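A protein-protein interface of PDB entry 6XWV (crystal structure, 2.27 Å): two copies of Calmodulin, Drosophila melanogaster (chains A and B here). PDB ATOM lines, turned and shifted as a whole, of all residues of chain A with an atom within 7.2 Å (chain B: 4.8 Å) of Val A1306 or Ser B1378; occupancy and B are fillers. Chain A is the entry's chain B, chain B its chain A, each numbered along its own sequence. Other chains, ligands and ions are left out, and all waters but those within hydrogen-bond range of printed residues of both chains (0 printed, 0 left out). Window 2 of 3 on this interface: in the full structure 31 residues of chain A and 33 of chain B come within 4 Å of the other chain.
O of Met B1385 sits at hydrogen-bond distance from N of Ser A1307.
O of Phe B1363 sits at hydrogen-bond distance from N of Leu B1380, at 2.8 Å.
N of Ser B1378 sits at hydrogen-bond distance from O of Val B1365, 2.7 Å away.
OG of Ser A1307 sits at hydrogen-bond distance from N of Asn A1326, 3.1 Å away.
Among the printed residues, pairs that only touch across the chains: Ser A1305 with Ile B1386 (3.3 Å), Val A1306 with Ser B1378 (3.5 Å), Val A1306 with Leu B1380 (3.6 Å), Val A1306 with Met B1385 (3.6 Å) and Val A1306 with Ile B1386 (3.9 Å).
Of the printed residues of chain B, Ser A1305 touches Ile B1386 (3.3 Å).
Of chain B, only Ser B1378, Leu B1380, Met B1385 and Ile B1386 come within 4 Å of Val A1306.
Glu A1311 touches none of the printed residues of chain B.
Thr B1367 touches none of the printed residues of chain A.
Of chain A, only Val A1306 (3.5 Å) comes within 4 Å of Ser B1378.
Of the printed residues of chain A, Met B1385 touches Val A1306 and Ser A1307.
Hydrophobic or aromatic side chains of chain A within 4 Å of the printed part of chain B: Val A1306.
Along chain A the printed residues that touch a printed residue of chain B span positions 1305 to 1307.
Of the 11 printed residues of chain B, 4 touch a printed residue of chain A.
Hydrophobic or aromatic side chains of chain B within 4 Å of the printed part of chain A: Leu B1380, Met B1385 and Ile B1386.
Among the printed residues, 6 pairs touch across the chains.
No position is printed for both chains.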
ATOM      1  N   SER A1305      28.507 -27.447  -9.072  1.00  0.00           N
ATOM      2  CA  SER A1305      28.187 -26.028  -8.965  1.00  0.00           C
ATOM      3  C   SER A1305      27.702 -25.471 -10.301  1.00  0.00           C
ATOM      4  O   SER A1305      28.287 -24.535 -10.850  1.00  0.00           O
ATOM      5  CB  SER A1305      29.403 -25.240  -8.475  1.00  0.00           C
ATOM      6  OG  SER A1305      30.609 -25.806  -8.955  1.00  0.00           O
ATOM      7  N   VAL A1306      26.624 -26.060 -10.816  1.00  0.00           N
ATOM      8  CA  VAL A1306      26.007 -25.644 -12.071  1.00  0.00           C
ATOM      9  C   VAL A1306      24.826 -24.737 -11.761  1.00  0.00           C
ATOM     10  O   VAL A1306      23.927 -25.115 -10.999  1.00  0.00           O
ATOM     11  CB  VAL A1306      25.556 -26.858 -12.899  1.00  0.00           C
ATOM     12  CG1 VAL A1306      24.621 -26.419 -14.015  1.00  0.00           C
ATOM     13  CG2 VAL A1306      26.757 -27.576 -13.468  1.00  0.00           C
ATOM     14  N   SER A1307      24.829 -23.544 -12.343  1.00  0.00           N
ATOM     15  CA  SER A1307      23.717 -22.601 -12.245  1.00  0.00           C
ATOM     16  C   SER A1307      23.101 -22.523 -13.639  1.00  0.00           C
ATOM     17  O   SER A1307      23.635 -21.854 -14.530  1.00  0.00           O
ATOM     18  CB  SER A1307      24.189 -21.237 -11.750  1.00  0.00           C
ATOM     19  OG  SER A1307      23.103 -20.334 -11.609  1.00  0.00           O
ATOM     20  N   SER A1308      21.989 -23.228 -13.833  1.00  0.00           N
ATOM     21  CA  SER A1308      21.402 -23.329 -15.159  1.00  0.00           C
ATOM     22  C   SER A1308      20.496 -22.139 -15.460  1.00  0.00           C
ATOM     23  O   SER A1308      20.121 -21.358 -14.581  1.00  0.00           O
ATOM     24  CB  SER A1308      20.615 -24.632 -15.311  1.00  0.00           C
ATOM     25  OG  SER A1308      19.682 -24.799 -14.263  1.00  0.00           O
ATOM     26  N   ALA A1309      20.163 -22.005 -16.747  1.00  0.00           N
ATOM     27  CA  ALA A1309      19.330 -20.895 -17.199  1.00  0.00           C
ATOM     28  C   ALA A1309      17.907 -20.958 -16.644  1.00  0.00           C
ATOM     29  O   ALA A1309      17.277 -19.911 -16.452  1.00  0.00           O
ATOM     30  CB  ALA A1309      19.298 -20.853 -18.728  1.00  0.00           C
ATOM     31  N   GLU A1311      17.094 -21.492 -13.724  1.00  0.00           N
ATOM     32  CA  GLU A1311      17.128 -20.955 -12.369  1.00  0.00           C
ATOM     33  C   GLU A1311      17.318 -19.452 -12.364  1.00  0.00           C
ATOM     34  O   GLU A1311      17.615 -18.865 -11.314  1.00  0.00           O
ATOM     35  CB  GLU A1311      18.241 -21.625 -11.558  1.00  0.00           C
ATOM     36  CG  GLU A1311      18.401 -23.099 -11.870  1.00  0.00           C
ATOM     37  CD  GLU A1311      19.600 -23.733 -11.187  1.00  0.00           C
ATOM     38  OE1 GLU A1311      20.396 -24.395 -11.888  1.00  0.00           O
ATOM     39  OE2 GLU A1311      19.753 -23.577  -9.957  1.00  0.00           O
ATOM     40  N   ASN A1326      23.425 -17.855  -9.698  1.00  0.00           N
ATOM     41  CA  ASN A1326      23.839 -18.144  -8.332  1.00  0.00           C
ATOM     42  C   ASN A1326      25.327 -18.470  -8.333  1.00  0.00           C
ATOM     43  O   ASN A1326      25.746 -19.506  -8.855  1.00  0.00           O
ATOM     44  CB  ASN A1326      23.041 -19.297  -7.738  1.00  0.00           C
ATOM     45  CG  ASN A1326      23.528 -19.674  -6.338  1.00  0.00           C
ATOM     46  OD1 ASN A1326      23.123 -19.068  -5.343  1.00  0.00           O
ATOM     47  ND2 ASN A1326      24.404 -20.668  -6.260  1.00  0.00           N
ATOM     48  N   PHE B1363      27.691 -29.070 -23.604  1.00  0.00           N
ATOM     49  CA  PHE B1363      29.003 -29.450 -23.107  1.00  0.00           C
ATOM     50  C   PHE B1363      28.871 -30.379 -21.910  1.00  0.00           C
ATOM     51  O   PHE B1363      27.943 -30.261 -21.106  1.00  0.00           O
ATOM     52  CB  PHE B1363      29.828 -28.232 -22.681  1.00  0.00           C
ATOM     53  CG  PHE B1363      30.363 -27.420 -23.822  1.00  0.00           C
ATOM     54  CD1 PHE B1363      31.521 -27.797 -24.477  1.00  0.00           C
ATOM     55  CD2 PHE B1363      29.717 -26.257 -24.226  1.00  0.00           C
ATOM     56  CE1 PHE B1363      32.025 -27.044 -25.521  1.00  0.00           C
ATOM     57  CE2 PHE B1363      30.215 -25.496 -25.272  1.00  0.00           C
ATOM     58  CZ  PHE B1363      31.372 -25.890 -25.919  1.00  0.00           C
ATOM     59  N   ASN B1364      29.832 -31.292 -21.797  1.00  0.00           N
ATOM     60  CA  ASN B1364      30.020 -32.145 -20.630  1.00  0.00           C
ATOM     61  C   ASN B1364      31.265 -31.652 -19.911  1.00  0.00           C
ATOM     62  O   ASN B1364      32.352 -31.630 -20.498  1.00  0.00           O
ATOM     63  CB  ASN B1364      30.179 -33.612 -21.027  1.00  0.00           C
ATOM     64  CG  ASN B1364      28.905 -34.211 -21.588  1.00  0.00           C
ATOM     65  OD1 ASN B1364      27.804 -33.950 -21.094  1.00  0.00           O
ATOM     66  ND2 ASN B1364      29.047 -35.015 -22.634  1.00  0.00           N
ATOM     67  N   VAL B1365      31.116 -31.268 -18.648  1.00  0.00           N
ATOM     68  CA  VAL B1365      32.220 -30.737 -17.859  1.00  0.00           C
ATOM     69  C   VAL B1365      32.484 -31.674 -16.690  1.00  0.00           C
ATOM     70  O   VAL B1365      31.553 -32.060 -15.971  1.00  0.00           O
ATOM     71  CB  VAL B1365      31.932 -29.312 -17.357  1.00  0.00           C
ATOM     72  CG1 VAL B1365      33.083 -28.815 -16.499  1.00  0.00           C
ATOM     73  CG2 VAL B1365      31.673 -28.366 -18.536  1.00  0.00           C
ATOM     74  N   THR B1367      34.718 -31.868 -13.181  1.00  0.00           N
ATOM     75  CA  THR B1367      35.406 -31.005 -12.233  1.00  0.00           C
ATOM     76  C   THR B1367      36.015 -31.848 -11.122  1.00  0.00           C
ATOM     77  O   THR B1367      35.369 -32.760 -10.596  1.00  0.00           O
ATOM     78  CB  THR B1367      34.445 -29.963 -11.640  1.00  0.00           C
ATOM     79  OG1 THR B1367      33.155 -30.558 -11.439  1.00  0.00           O
ATOM     80  CG2 THR B1367      34.302 -28.769 -12.577  1.00  0.00           C
ATOM     81  N   VAL B1376      33.364 -34.653 -10.402  1.00  0.00           N
ATOM     82  CA  VAL B1376      31.975 -34.256 -10.578  1.00  0.00           C
ATOM     83  C   VAL B1376      31.718 -34.047 -12.061  1.00  0.00           C
ATOM     84  O   VAL B1376      32.529 -33.438 -12.766  1.00  0.00           O
ATOM     85  CB  VAL B1376      31.672 -32.981  -9.768  1.00  0.00           C
ATOM     86  CG1 VAL B1376      30.290 -32.434 -10.104  1.00  0.00           C
ATOM     87  CG2 VAL B1376      31.806 -33.256  -8.277  1.00  0.00           C
ATOM     88  N   HIS B1377      30.590 -34.562 -12.540  1.00  0.00           N
ATOM     89  CA  HIS B1377      30.225 -34.493 -13.947  1.00  0.00           C
ATOM     90  C   HIS B1377      29.031 -33.564 -14.103  1.00  0.00           C
ATOM     91  O   HIS B1377      28.043 -33.688 -13.372  1.00  0.00           O
ATOM     92  CB  HIS B1377      29.901 -35.884 -14.497  1.00  0.00           C
ATOM     93  CG  HIS B1377      29.133 -35.862 -15.780  1.00  0.00           C
ATOM     94  ND1 HIS B1377      29.575 -35.186 -16.896  1.00  0.00           N
ATOM     95  CD2 HIS B1377      27.960 -36.442 -16.131  1.00  0.00           C
ATOM     96  CE1 HIS B1377      28.705 -35.342 -17.876  1.00  0.00           C
ATOM     97  NE2 HIS B1377      27.717 -36.101 -17.439  1.00  0.00           N
ATOM     98  N   SER B1378      29.127 -32.636 -15.052  1.00  0.00           N
ATOM     99  CA  SER B1378      28.074 -31.663 -15.298  1.00  0.00           C
ATOM    100  C   SER B1378      27.754 -31.611 -16.783  1.00  0.00           C
ATOM    101  O   SER B1378      28.649 -31.711 -17.629  1.00  0.00           O
ATOM    102  CB  SER B1378      28.481 -30.274 -14.810  1.00  0.00           C
ATOM    103  OG  SER B1378      29.203 -30.356 -13.593  1.00  0.00           O
ATOM    104  N   VAL B1379      26.473 -31.449 -17.091  1.00  0.00           N
ATOM    105  CA  VAL B1379      26.007 -31.238 -18.455  1.00  0.00           C
ATOM    106  C   VAL B1379      25.479 -29.815 -18.541  1.00  0.00           C
ATOM    107  O   VAL B1379      24.620 -29.412 -17.749  1.00  0.00           O
ATOM    108  CB  VAL B1379      24.922 -32.250 -18.850  1.00  0.00           C
ATOM    109  CG1 VAL B1379      24.480 -32.017 -20.293  1.00  0.00           C
ATOM    110  CG2 VAL B1379      25.427 -33.680 -18.654  1.00  0.00           C
ATOM    111  N   LEU B1380      25.987 -29.054 -19.498  1.00  0.00           N
ATOM    112  CA  LEU B1380      25.621 -27.658 -19.658  1.00  0.00           C
ATOM    113  C   LEU B1380      25.054 -27.465 -21.059  1.00  0.00           C
ATOM    114  O   LEU B1380      25.739 -27.738 -22.051  1.00  0.00           O
ATOM    115  CB  LEU B1380      26.846 -26.766 -19.451  1.00  0.00           C
ATOM    116  CG  LEU B1380      27.539 -26.695 -18.085  1.00  0.00           C
ATOM    117  CD1 LEU B1380      28.762 -25.782 -18.124  1.00  0.00           C
ATOM    118  CD2 LEU B1380      26.580 -26.234 -17.004  1.00  0.00           C
ATOM    119  N   MET B1385      25.767 -22.086 -16.772  1.00  0.00           N
ATOM    120  CA  MET B1385      27.057 -21.585 -16.327  1.00  0.00           C
ATOM    121  C   MET B1385      27.565 -22.456 -15.191  1.00  0.00           C
ATOM    122  O   MET B1385      26.784 -22.921 -14.357  1.00  0.00           O
ATOM    123  CB  MET B1385      26.961 -20.124 -15.868  1.00  0.00           C
ATOM    124  CG  MET B1385      28.298 -19.484 -15.523  1.00  0.00           C
ATOM    125  SD  MET B1385      28.695 -19.609 -13.770  1.00  0.00           S
ATOM    126  CE  MET B1385      27.507 -18.479 -13.081  1.00  0.00           C
ATOM    127  N   ILE B1386      28.878 -22.660 -15.155  1.00  0.00           N
ATOM    128  CA  ILE B1386      29.534 -23.373 -14.067  1.00  0.00           C
ATOM    129  C   ILE B1386      30.693 -22.521 -13.564  1.00  0.00           C
ATOM    130  O   ILE B1386      31.396 -21.876 -14.348  1.00  0.00           O
ATOM    131  CB  ILE B1386      29.998 -24.785 -14.499  1.00  0.00           C
ATOM    132  CG1 ILE B1386      30.199 -25.680 -13.272  1.00  0.00           C
ATOM    133  CG2 ILE B1386      31.254 -24.729 -15.354  1.00  0.00           C
ATOM    134  CD1 ILE B1386      30.787 -27.039 -13.591  1.00  0.00           C
